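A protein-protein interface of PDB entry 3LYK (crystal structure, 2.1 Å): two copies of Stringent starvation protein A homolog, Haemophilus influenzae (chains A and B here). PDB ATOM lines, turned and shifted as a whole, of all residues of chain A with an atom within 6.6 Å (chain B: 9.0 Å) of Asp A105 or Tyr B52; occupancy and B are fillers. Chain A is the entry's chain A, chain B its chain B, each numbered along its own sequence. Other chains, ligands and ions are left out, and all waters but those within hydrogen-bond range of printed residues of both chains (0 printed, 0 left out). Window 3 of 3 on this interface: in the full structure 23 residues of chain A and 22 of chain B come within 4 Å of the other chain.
The guanidinium group (NE) of Arg A101 is in hydrogen-bond range of the side-chain hydroxyl (OH) of Tyr B52 (2.8 Å).
OD2 of Asp A105 sits at hydrogen-bond distance from OH of Tyr B52 (2.7 Å).
The side-chain amide nitrogen (NE2) of Gln A104 is in hydrogen-bond range of the side-chain carboxylate (OD1) of Asp A105, 3.2 Å away.
The side-chain amide oxygen (OD1) of Asn B50 is in hydrogen-bond range of the backbone NH (N) of Tyr B52 (3.1 Å).
CB of Asn B67 touches CD2 of Leu A100 (3.7 Å).
Tyr B52 touches Gln A104 (CE1 to NE2, 3.4 Å).
Of the printed residues of chain B, Arg A101 touches Tyr B52 (2.8 Å).
Of the printed residues of chain B, Gln A104 touches Tyr B52.
Asp A105 touches just one residue of chain B: Tyr B52 (2.7 Å).
Tyr B52 touches just these residues of chain A: Arg A101, Gln A104 and Asp A105.
Thr B57 touches none of the printed residues of chain A.
Leu B65 touches none of the printed residues of chain A.
Of the printed residues of chain A, Asn B67 touches Leu A100 (3.7 Å).
The nearest residue of chain B that does not touch Asp A105 is Phe B66 (7.7 Å).
Of the 16 printed residues of chain B, 2 touch a printed residue of chain A.
Of the 14 printed residues of chain A, 4 touch a printed residue of chain B.
Printed residues of chain A that touch a printed residue of chain B: Leu A100, Arg A101, Gln A104 and Asp A105.
Among the printed residues, 4 pairs touch across the chains.
No position is printed for both chains.
Of the 4 pairs that touch across the chains among the printed residues, none has its exchanged pair printed and touching as well.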
ATOM      1  N   LEU A 100     -18.779  10.772 -11.326  1.00  0.00           N
ATOM      2  CA  LEU A 100     -19.261   9.694 -12.190  1.00  0.00           C
ATOM      3  C   LEU A 100     -20.670   9.240 -11.755  1.00  0.00           C
ATOM      4  O   LEU A 100     -21.555   9.082 -12.589  1.00  0.00           O
ATOM      5  CB  LEU A 100     -18.272   8.501 -12.195  1.00  0.00           C
ATOM      6  CG  LEU A 100     -18.741   7.289 -13.020  1.00  0.00           C
ATOM      7  CD1 LEU A 100     -18.670   7.609 -14.514  1.00  0.00           C
ATOM      8  CD2 LEU A 100     -17.888   6.032 -12.723  1.00  0.00           C
ATOM      9  N   ARG A 101     -20.873   9.071 -10.466  1.00  0.00           N
ATOM     10  CA  ARG A 101     -22.130   8.579  -9.920  1.00  0.00           C
ATOM     11  C   ARG A 101     -23.290   9.599 -10.041  1.00  0.00           C
ATOM     12  O   ARG A 101     -24.428   9.222 -10.395  1.00  0.00           O
ATOM     13  CB  ARG A 101     -21.929   8.209  -8.466  1.00  0.00           C
ATOM     14  CG  ARG A 101     -21.114   6.867  -8.309  1.00  0.00           C
ATOM     15  CD  ARG A 101     -20.932   6.473  -6.830  1.00  0.00           C
ATOM     16  NE  ARG A 101     -22.221   6.597  -6.152  1.00  0.00           N
ATOM     17  CZ  ARG A 101     -22.466   7.360  -5.083  1.00  0.00           C
ATOM     18  NH1 ARG A 101     -21.493   8.052  -4.496  1.00  0.00           N
ATOM     19  NH2 ARG A 101     -23.705   7.434  -4.598  1.00  0.00           N
ATOM     20  N   ILE A 102     -22.995  10.864  -9.731  1.00  0.00           N
ATOM     21  CA  ILE A 102     -23.932  11.953 -10.016  1.00  0.00           C
ATOM     22  C   ILE A 102     -24.395  11.929 -11.461  1.00  0.00           C
ATOM     23  O   ILE A 102     -25.593  11.868 -11.726  1.00  0.00           O
ATOM     24  CB  ILE A 102     -23.361  13.337  -9.613  1.00  0.00           C
ATOM     25  CG1 ILE A 102     -23.252  13.405  -8.074  1.00  0.00           C
ATOM     26  CG2 ILE A 102     -24.260  14.482 -10.181  1.00  0.00           C
ATOM     27  CD1 ILE A 102     -22.186  14.347  -7.557  1.00  0.00           C
ATOM     28  N   GLU A 103     -23.460  11.956 -12.400  1.00  0.00           N
ATOM     29  CA  GLU A 103     -23.805  11.999 -13.802  1.00  0.00           C
ATOM     30  C   GLU A 103     -24.568  10.733 -14.291  1.00  0.00           C
ATOM     31  O   GLU A 103     -25.457  10.801 -15.170  1.00  0.00           O
ATOM     32  CB  GLU A 103     -22.532  12.209 -14.608  1.00  0.00           C
ATOM     33  CG  GLU A 103     -22.675  12.802 -15.970  1.00  0.00           C
ATOM     34  CD  GLU A 103     -23.051  11.767 -17.024  1.00  0.00           C
ATOM     35  OE1 GLU A 103     -23.336  12.156 -18.184  1.00  0.00           O
ATOM     36  OE2 GLU A 103     -23.054  10.556 -16.708  1.00  0.00           O
ATOM     37  N   GLN A 104     -24.232   9.588 -13.728  1.00  0.00           N
ATOM     38  CA  GLN A 104     -24.805   8.330 -14.200  1.00  0.00           C
ATOM     39  C   GLN A 104     -26.173   8.072 -13.573  1.00  0.00           C
ATOM     40  O   GLN A 104     -27.074   7.547 -14.231  1.00  0.00           O
ATOM     41  CB  GLN A 104     -23.810   7.185 -13.892  1.00  0.00           C
ATOM     42  CG  GLN A 104     -24.337   5.761 -14.010  1.00  0.00           C
ATOM     43  CD  GLN A 104     -23.290   4.750 -13.485  1.00  0.00           C
ATOM     44  OE1 GLN A 104     -22.205   4.597 -14.074  1.00  0.00           O
ATOM     45  NE2 GLN A 104     -23.592   4.122 -12.343  1.00  0.00           N
ATOM     46  N   ASP A 105     -26.322   8.423 -12.305  1.00  0.00           N
ATOM     47  CA  ASP A 105     -27.522   8.118 -11.583  1.00  0.00           C
ATOM     48  C   ASP A 105     -28.563   9.255 -11.564  1.00  0.00           C
ATOM     49  O   ASP A 105     -29.756   8.968 -11.518  1.00  0.00           O
ATOM     50  CB  ASP A 105     -27.201   7.759 -10.148  1.00  0.00           C
ATOM     51  CG  ASP A 105     -26.318   6.519 -10.021  1.00  0.00           C
ATOM     52  OD1 ASP A 105     -26.000   5.855 -11.044  1.00  0.00           O
ATOM     53  OD2 ASP A 105     -25.964   6.220  -8.867  1.00  0.00           O
ATOM     54  N   TRP A 106     -28.112  10.519 -11.532  1.00  0.00           N
ATOM     55  CA  TRP A 106     -29.036  11.679 -11.387  1.00  0.00           C
ATOM     56  C   TRP A 106     -29.353  12.370 -12.700  1.00  0.00           C
ATOM     57  O   TRP A 106     -30.489  12.757 -12.948  1.00  0.00           O
ATOM     58  CB  TRP A 106     -28.488  12.691 -10.384  1.00  0.00           C
ATOM     59  CG  TRP A 106     -28.510  12.193  -8.987  1.00  0.00           C
ATOM     60  CD1 TRP A 106     -29.141  11.067  -8.517  1.00  0.00           C
ATOM     61  CD2 TRP A 106     -27.925  12.820  -7.848  1.00  0.00           C
ATOM     62  NE1 TRP A 106     -28.955  10.943  -7.161  1.00  0.00           N
ATOM     63  CE2 TRP A 106     -28.211  12.006  -6.724  1.00  0.00           C
ATOM     64  CE3 TRP A 106     -27.182  13.995  -7.661  1.00  0.00           C
ATOM     65  CZ2 TRP A 106     -27.773  12.335  -5.432  1.00  0.00           C
ATOM     66  CZ3 TRP A 106     -26.738  14.317  -6.376  1.00  0.00           C
ATOM     67  CH2 TRP A 106     -27.023  13.486  -5.287  1.00  0.00           C
ATOM     68  N   TYR A 107     -28.365  12.500 -13.568  1.00  0.00           N
ATOM     69  CA  TYR A 107     -28.573  13.233 -14.787  1.00  0.00           C
ATOM     70  C   TYR A 107     -29.659  12.679 -15.730  1.00  0.00           C
ATOM     71  O   TYR A 107     -30.363  13.505 -16.355  1.00  0.00           O
ATOM     72  CB  TYR A 107     -27.265  13.511 -15.519  1.00  0.00           C
ATOM     73  CG  TYR A 107     -26.447  14.694 -14.949  1.00  0.00           C
ATOM     74  CD1 TYR A 107     -26.560  15.091 -13.623  1.00  0.00           C
ATOM     75  CD2 TYR A 107     -25.579  15.412 -15.774  1.00  0.00           C
ATOM     76  CE1 TYR A 107     -25.789  16.174 -13.110  1.00  0.00           C
ATOM     77  CE2 TYR A 107     -24.830  16.482 -15.293  1.00  0.00           C
ATOM     78  CZ  TYR A 107     -24.931  16.842 -13.960  1.00  0.00           C
ATOM     79  OH  TYR A 107     -24.164  17.914 -13.520  1.00  0.00           O
ATOM     80  N   PRO A 108     -29.782  11.317 -15.876  1.00  0.00           N
ATOM     81  CA  PRO A 108     -30.846  10.804 -16.775  1.00  0.00           C
ATOM     82  C   PRO A 108     -32.264  11.118 -16.292  1.00  0.00           C
ATOM     83  O   PRO A 108     -33.136  11.396 -17.105  1.00  0.00           O
ATOM     84  CB  PRO A 108     -30.603   9.281 -16.804  1.00  0.00           C
ATOM     85  CG  PRO A 108     -29.078   9.166 -16.575  1.00  0.00           C
ATOM     86  CD  PRO A 108     -28.793  10.257 -15.542  1.00  0.00           C
ATOM     87  N   THR A 109     -32.472  11.080 -14.988  1.00  0.00           N
ATOM     88  CA  THR A 109     -33.724  11.451 -14.390  1.00  0.00           C
ATOM     89  C   THR A 109     -34.008  12.947 -14.632  1.00  0.00           C
ATOM     90  O   THR A 109     -35.157  13.313 -14.849  1.00  0.00           O
ATOM     91  CB  THR A 109     -33.729  11.126 -12.894  1.00  0.00           C
ATOM     92  OG1 THR A 109     -33.463   9.728 -12.736  1.00  0.00           O
ATOM     93  CG2 THR A 109     -35.076  11.409 -12.249  1.00  0.00           C
ATOM     94  N   LEU A 110     -32.959  13.776 -14.649  1.00  0.00           N
ATOM     95  CA  LEU A 110     -33.105  15.201 -14.924  1.00  0.00           C
ATOM     96  C   LEU A 110     -33.474  15.433 -16.380  1.00  0.00           C
ATOM     97  O   LEU A 110     -34.345  16.254 -16.647  1.00  0.00           O
ATOM     98  CB  LEU A 110     -31.869  15.999 -14.494  1.00  0.00           C
ATOM     99  CG  LEU A 110     -31.806  17.500 -14.754  1.00  0.00           C
ATOM    100  CD1 LEU A 110     -32.871  18.290 -13.935  1.00  0.00           C
ATOM    101  CD2 LEU A 110     -30.416  18.038 -14.460  1.00  0.00           C
ATOM    102  N   GLN A 127     -39.062  11.790  -8.061  1.00  0.00           N
ATOM    103  CA  GLN A 127     -37.910  10.926  -7.794  1.00  0.00           C
ATOM    104  C   GLN A 127     -36.668  11.752  -7.364  1.00  0.00           C
ATOM    105  O   GLN A 127     -36.152  11.563  -6.257  1.00  0.00           O
ATOM    106  CB  GLN A 127     -37.604  10.046  -9.008  1.00  0.00           C
ATOM    107  CG  GLN A 127     -36.920   8.705  -8.651  1.00  0.00           C
ATOM    108  CD  GLN A 127     -36.084   8.121  -9.807  1.00  0.00           C
ATOM    109  OE1 GLN A 127     -36.598   7.864 -10.906  1.00  0.00           O
ATOM    110  NE2 GLN A 127     -34.789   7.905  -9.551  1.00  0.00           N
ATOM    111  N   LEU A 128     -36.229  12.688  -8.215  1.00  0.00           N
ATOM    112  CA  LEU A 128     -35.046  13.532  -7.921  1.00  0.00           C
ATOM    113  C   LEU A 128     -35.168  14.260  -6.602  1.00  0.00           C
ATOM    114  O   LEU A 128     -34.295  14.174  -5.739  1.00  0.00           O
ATOM    115  CB  LEU A 128     -34.822  14.542  -9.024  1.00  0.00           C
ATOM    116  CG  LEU A 128     -33.940  14.056 -10.157  1.00  0.00           C
ATOM    117  CD1 LEU A 128     -33.820  15.121 -11.213  1.00  0.00           C
ATOM    118  CD2 LEU A 128     -32.565  13.684  -9.623  1.00  0.00           C
ATOM    119  N   GLU A 131     -34.675  11.623  -3.795  1.00  0.00           N
ATOM    120  CA  GLU A 131     -33.283  11.250  -3.540  1.00  0.00           C
ATOM    121  C   GLU A 131     -32.410  12.364  -2.959  1.00  0.00           C
ATOM    122  O   GLU A 131     -31.521  12.105  -2.150  1.00  0.00           O
ATOM    123  CB  GLU A 131     -32.613  10.534  -4.736  1.00  0.00           C
ATOM    124  CG  GLU A 131     -33.159  10.828  -6.134  1.00  0.00           C
ATOM    125  CD  GLU A 131     -33.046   9.620  -7.082  1.00  0.00           C
ATOM    126  OE1 GLU A 131     -33.234   8.488  -6.586  1.00  0.00           O
ATOM    127  OE2 GLU A 131     -32.791   9.795  -8.314  1.00  0.00           O
ATOM    128  N   LEU B  42     -21.920 -13.016  -9.316  1.00  0.00           N
ATOM    129  CA  LEU B  42     -21.020 -12.066  -8.654  1.00  0.00           C
ATOM    130  C   LEU B  42     -20.888 -12.448  -7.214  1.00  0.00           C
ATOM    131  O   LEU B  42     -21.853 -12.881  -6.638  1.00  0.00           O
ATOM    132  CB  LEU B  42     -21.603 -10.627  -8.762  1.00  0.00           C
ATOM    133  CG  LEU B  42     -21.769 -10.157 -10.206  1.00  0.00           C
ATOM    134  CD1 LEU B  42     -22.558  -8.812 -10.277  1.00  0.00           C
ATOM    135  CD2 LEU B  42     -20.401 -10.044 -10.892  1.00  0.00           C
ATOM    136  N   LEU B  46     -18.111  -8.499  -3.266  1.00  0.00           N
ATOM    137  CA  LEU B  46     -18.102  -7.417  -4.250  1.00  0.00           C
ATOM    138  C   LEU B  46     -19.361  -6.549  -4.136  1.00  0.00           C
ATOM    139  O   LEU B  46     -19.253  -5.309  -4.158  1.00  0.00           O
ATOM    140  CB  LEU B  46     -17.937  -7.905  -5.703  1.00  0.00           C
ATOM    141  CG  LEU B  46     -18.033  -6.822  -6.801  1.00  0.00           C
ATOM    142  CD1 LEU B  46     -16.926  -5.774  -6.649  1.00  0.00           C
ATOM    143  CD2 LEU B  46     -18.013  -7.398  -8.196  1.00  0.00           C
ATOM    144  N   MET B  47     -20.539  -7.184  -4.055  1.00  0.00           N
ATOM    145  CA  MET B  47     -21.817  -6.442  -3.884  1.00  0.00           C
ATOM    146  C   MET B  47     -21.855  -5.520  -2.641  1.00  0.00           C
ATOM    147  O   MET B  47     -22.378  -4.431  -2.713  1.00  0.00           O
ATOM    148  CB  MET B  47     -23.025  -7.393  -3.841  1.00  0.00           C
ATOM    149  CG  MET B  47     -23.090  -8.348  -5.019  1.00  0.00           C
ATOM    150  SD  MET B  47     -23.041  -7.438  -6.751  1.00  0.00           S
ATOM    151  CE  MET B  47     -24.428  -6.036  -6.514  1.00  0.00           C
ATOM    152  N   GLU B  48     -21.309  -5.999  -1.533  1.00  0.00           N
ATOM    153  CA  GLU B  48     -21.132  -5.269  -0.288  1.00  0.00           C
ATOM    154  C   GLU B  48     -20.280  -3.988  -0.486  1.00  0.00           C
ATOM    155  O   GLU B  48     -20.607  -2.932   0.054  1.00  0.00           O
ATOM    156  CB  GLU B  48     -20.390  -6.186   0.672  1.00  0.00           C
ATOM    157  CG  GLU B  48     -20.989  -6.368   2.047  1.00  0.00           C
ATOM    158  CD  GLU B  48     -20.700  -7.786   2.604  1.00  0.00           C
ATOM    159  OE1 GLU B  48     -21.683  -8.549   2.843  1.00  0.00           O
ATOM    160  OE2 GLU B  48     -19.497  -8.156   2.765  1.00  0.00           O
ATOM    161  N   LEU B  49     -19.208  -4.094  -1.273  1.00  0.00           N
ATOM    162  CA  LEU B  49     -18.241  -3.020  -1.446  1.00  0.00           C
ATOM    163  C   LEU B  49     -18.622  -2.091  -2.598  1.00  0.00           C
ATOM    164  O   LEU B  49     -18.399  -0.891  -2.514  1.00  0.00           O
ATOM    165  CB  LEU B  49     -16.831  -3.593  -1.640  1.00  0.00           C
ATOM    166  CG  LEU B  49     -16.246  -4.415  -0.481  1.00  0.00           C
ATOM    167  CD1 LEU B  49     -15.074  -5.290  -0.910  1.00  0.00           C
ATOM    168  CD2 LEU B  49     -15.835  -3.540   0.705  1.00  0.00           C
ATOM    169  N   ASN B  50     -19.195  -2.653  -3.664  1.00  0.00           N
ATOM    170  CA  ASN B  50     -19.583  -1.920  -4.863  1.00  0.00           C
ATOM    171  C   ASN B  50     -21.001  -2.338  -5.264  1.00  0.00           C
ATOM    172  O   ASN B  50     -21.188  -3.349  -5.951  1.00  0.00           O
ATOM    173  CB  ASN B  50     -18.575  -2.150  -6.022  1.00  0.00           C
ATOM    174  CG  ASN B  50     -19.018  -1.500  -7.337  1.00  0.00           C
ATOM    175  OD1 ASN B  50     -19.972  -0.718  -7.347  1.00  0.00           O
ATOM    176  ND2 ASN B  50     -18.316  -1.810  -8.461  1.00  0.00           N
ATOM    177  N   PRO B  51     -22.008  -1.519  -4.879  1.00  0.00           N
ATOM    178  CA  PRO B  51     -23.389  -1.937  -5.133  1.00  0.00           C
ATOM    179  C   PRO B  51     -23.764  -1.943  -6.613  1.00  0.00           C
ATOM    180  O   PRO B  51     -24.768  -2.550  -6.961  1.00  0.00           O
ATOM    181  CB  PRO B  51     -24.239  -0.955  -4.296  1.00  0.00           C
ATOM    182  CG  PRO B  51     -23.355   0.378  -4.266  1.00  0.00           C
ATOM    183  CD  PRO B  51     -21.917  -0.212  -4.165  1.00  0.00           C
ATOM    184  N   TYR B  52     -22.989  -1.308  -7.489  1.00  0.00           N
ATOM    185  CA  TYR B  52     -23.286  -1.412  -8.920  1.00  0.00           C
ATOM    186  C   TYR B  52     -22.876  -2.787  -9.452  1.00  0.00           C
ATOM    187  O   TYR B  52     -23.273  -3.170 -10.548  1.00  0.00           O
ATOM    188  CB  TYR B  52     -22.608  -0.308  -9.741  1.00  0.00           C
ATOM    189  CG  TYR B  52     -22.951   1.094  -9.240  1.00  0.00           C
ATOM    190  CD1 TYR B  52     -24.077   1.796  -9.730  1.00  0.00           C
ATOM    191  CD2 TYR B  52     -22.180   1.691  -8.252  1.00  0.00           C
ATOM    192  CE1 TYR B  52     -24.399   3.087  -9.247  1.00  0.00           C
ATOM    193  CE2 TYR B  52     -22.488   2.970  -7.757  1.00  0.00           C
ATOM    194  CZ  TYR B  52     -23.594   3.672  -8.258  1.00  0.00           C
ATOM    195  OH  TYR B  52     -23.850   4.940  -7.725  1.00  0.00           O
ATOM    196  N   GLY B  53     -22.060  -3.504  -8.684  1.00  0.00           N
ATOM    197  CA  GLY B  53     -21.617  -4.849  -9.054  1.00  0.00           C
ATOM    198  C   GLY B  53     -20.857  -4.917 -10.361  1.00  0.00           C
ATOM    199  O   GLY B  53     -21.116  -5.788 -11.164  1.00  0.00           O
ATOM    200  N   THR B  54     -19.939  -3.980 -10.591  1.00  0.00           N
ATOM    201  CA  THR B  54     -19.175  -3.956 -11.859  1.00  0.00           C
ATOM    202  C   THR B  54     -17.705  -4.330 -11.581  1.00  0.00           C
ATOM    203  O   THR B  54     -17.219  -4.244 -10.438  1.00  0.00           O
ATOM    204  CB  THR B  54     -19.175  -2.547 -12.493  1.00  0.00           C
ATOM    205  OG1 THR B  54     -18.701  -1.629 -11.512  1.00  0.00           O
ATOM    206  CG2 THR B  54     -20.607  -2.128 -12.971  1.00  0.00           C
ATOM    207  N   VAL B  55     -16.999  -4.740 -12.625  1.00  0.00           N
ATOM    208  CA  VAL B  55     -15.573  -4.922 -12.504  1.00  0.00           C
ATOM    209  C   VAL B  55     -14.946  -4.155 -13.646  1.00  0.00           C
ATOM    210  O   VAL B  55     -15.581  -3.958 -14.662  1.00  0.00           O
ATOM    211  CB  VAL B  55     -15.147  -6.439 -12.549  1.00  0.00           C
ATOM    212  CG1 VAL B  55     -15.559  -7.146 -11.237  1.00  0.00           C
ATOM    213  CG2 VAL B  55     -15.727  -7.149 -13.766  1.00  0.00           C
ATOM    214  N   THR B  57     -13.102  -3.557  -9.929  1.00  0.00           N
ATOM    215  CA  THR B  57     -13.254  -2.827  -8.693  1.00  0.00           C
ATOM    216  C   THR B  57     -11.964  -3.056  -7.892  1.00  0.00           C
ATOM    217  O   THR B  57     -11.546  -4.222  -7.694  1.00  0.00           O
ATOM    218  CB  THR B  57     -14.463  -3.343  -7.889  1.00  0.00           C
ATOM    219  OG1 THR B  57     -15.665  -3.013  -8.576  1.00  0.00           O
ATOM    220  CG2 THR B  57     -14.512  -2.728  -6.534  1.00  0.00           C
ATOM    221  N   VAL B  64     -12.782   2.126  -1.939  1.00  0.00           N
ATOM    222  CA  VAL B  64     -13.335   1.293  -3.014  1.00  0.00           C
ATOM    223  C   VAL B  64     -13.436   2.070  -4.322  1.00  0.00           C
ATOM    224  O   VAL B  64     -14.170   3.062  -4.408  1.00  0.00           O
ATOM    225  CB  VAL B  64     -14.742   0.689  -2.627  1.00  0.00           C
ATOM    226  CG1 VAL B  64     -15.373  -0.060  -3.826  1.00  0.00           C
ATOM    227  CG2 VAL B  64     -14.631  -0.209  -1.377  1.00  0.00           C
ATOM    228  N   LEU B  65     -12.725   1.640  -5.360  1.00  0.00           N
ATOM    229  CA  LEU B  65     -12.855   2.301  -6.670  1.00  0.00           C
ATOM    230  C   LEU B  65     -13.402   1.371  -7.746  1.00  0.00           C
ATOM    231  O   LEU B  65     -13.063   0.196  -7.761  1.00  0.00           O
ATOM    232  CB  LEU B  65     -11.477   2.818  -7.136  1.00  0.00           C
ATOM    233  CG  LEU B  65     -10.836   3.932  -6.302  1.00  0.00           C
ATOM    234  CD1 LEU B  65      -9.515   4.350  -6.937  1.00  0.00           C
ATOM    235  CD2 LEU B  65     -11.793   5.146  -6.195  1.00  0.00           C
ATOM    236  N   PHE B  66     -14.208   1.897  -8.668  1.00  0.00           N
ATOM    237  CA  PHE B  66     -14.566   1.160  -9.881  1.00  0.00           C
ATOM    238  C   PHE B  66     -14.500   2.163 -10.994  1.00  0.00           C
ATOM    239  O   PHE B  66     -14.256   3.367 -10.733  1.00  0.00           O
ATOM    240  CB  PHE B  66     -15.948   0.504  -9.783  1.00  0.00           C
ATOM    241  CG  PHE B  66     -17.018   1.421  -9.257  1.00  0.00           C
ATOM    242  CD1 PHE B  66     -17.783   2.187 -10.134  1.00  0.00           C
ATOM    243  CD2 PHE B  66     -17.219   1.552  -7.883  1.00  0.00           C
ATOM    244  CE1 PHE B  66     -18.769   3.054  -9.650  1.00  0.00           C
ATOM    245  CE2 PHE B  66     -18.212   2.418  -7.385  1.00  0.00           C
ATOM    246  CZ  PHE B  66     -18.973   3.166  -8.276  1.00  0.00           C
ATOM    247  N   ASN B  67     -14.736   1.700 -12.215  1.00  0.00           N
ATOM    248  CA  ASN B  67     -14.379   2.418 -13.443  1.00  0.00           C
ATOM    249  C   ASN B  67     -12.878   2.425 -13.685  1.00  0.00           C
ATOM    250  O   ASN B  67     -12.092   2.975 -12.894  1.00  0.00           O
ATOM    251  CB  ASN B  67     -14.950   3.860 -13.481  1.00  0.00           C
ATOM    252  CG  ASN B  67     -14.657   4.556 -14.779  1.00  0.00           C
ATOM    253  OD1 ASN B  67     -13.546   5.035 -14.993  1.00  0.00           O
ATOM    254  ND2 ASN B  67     -15.648   4.611 -15.671  1.00  0.00           N
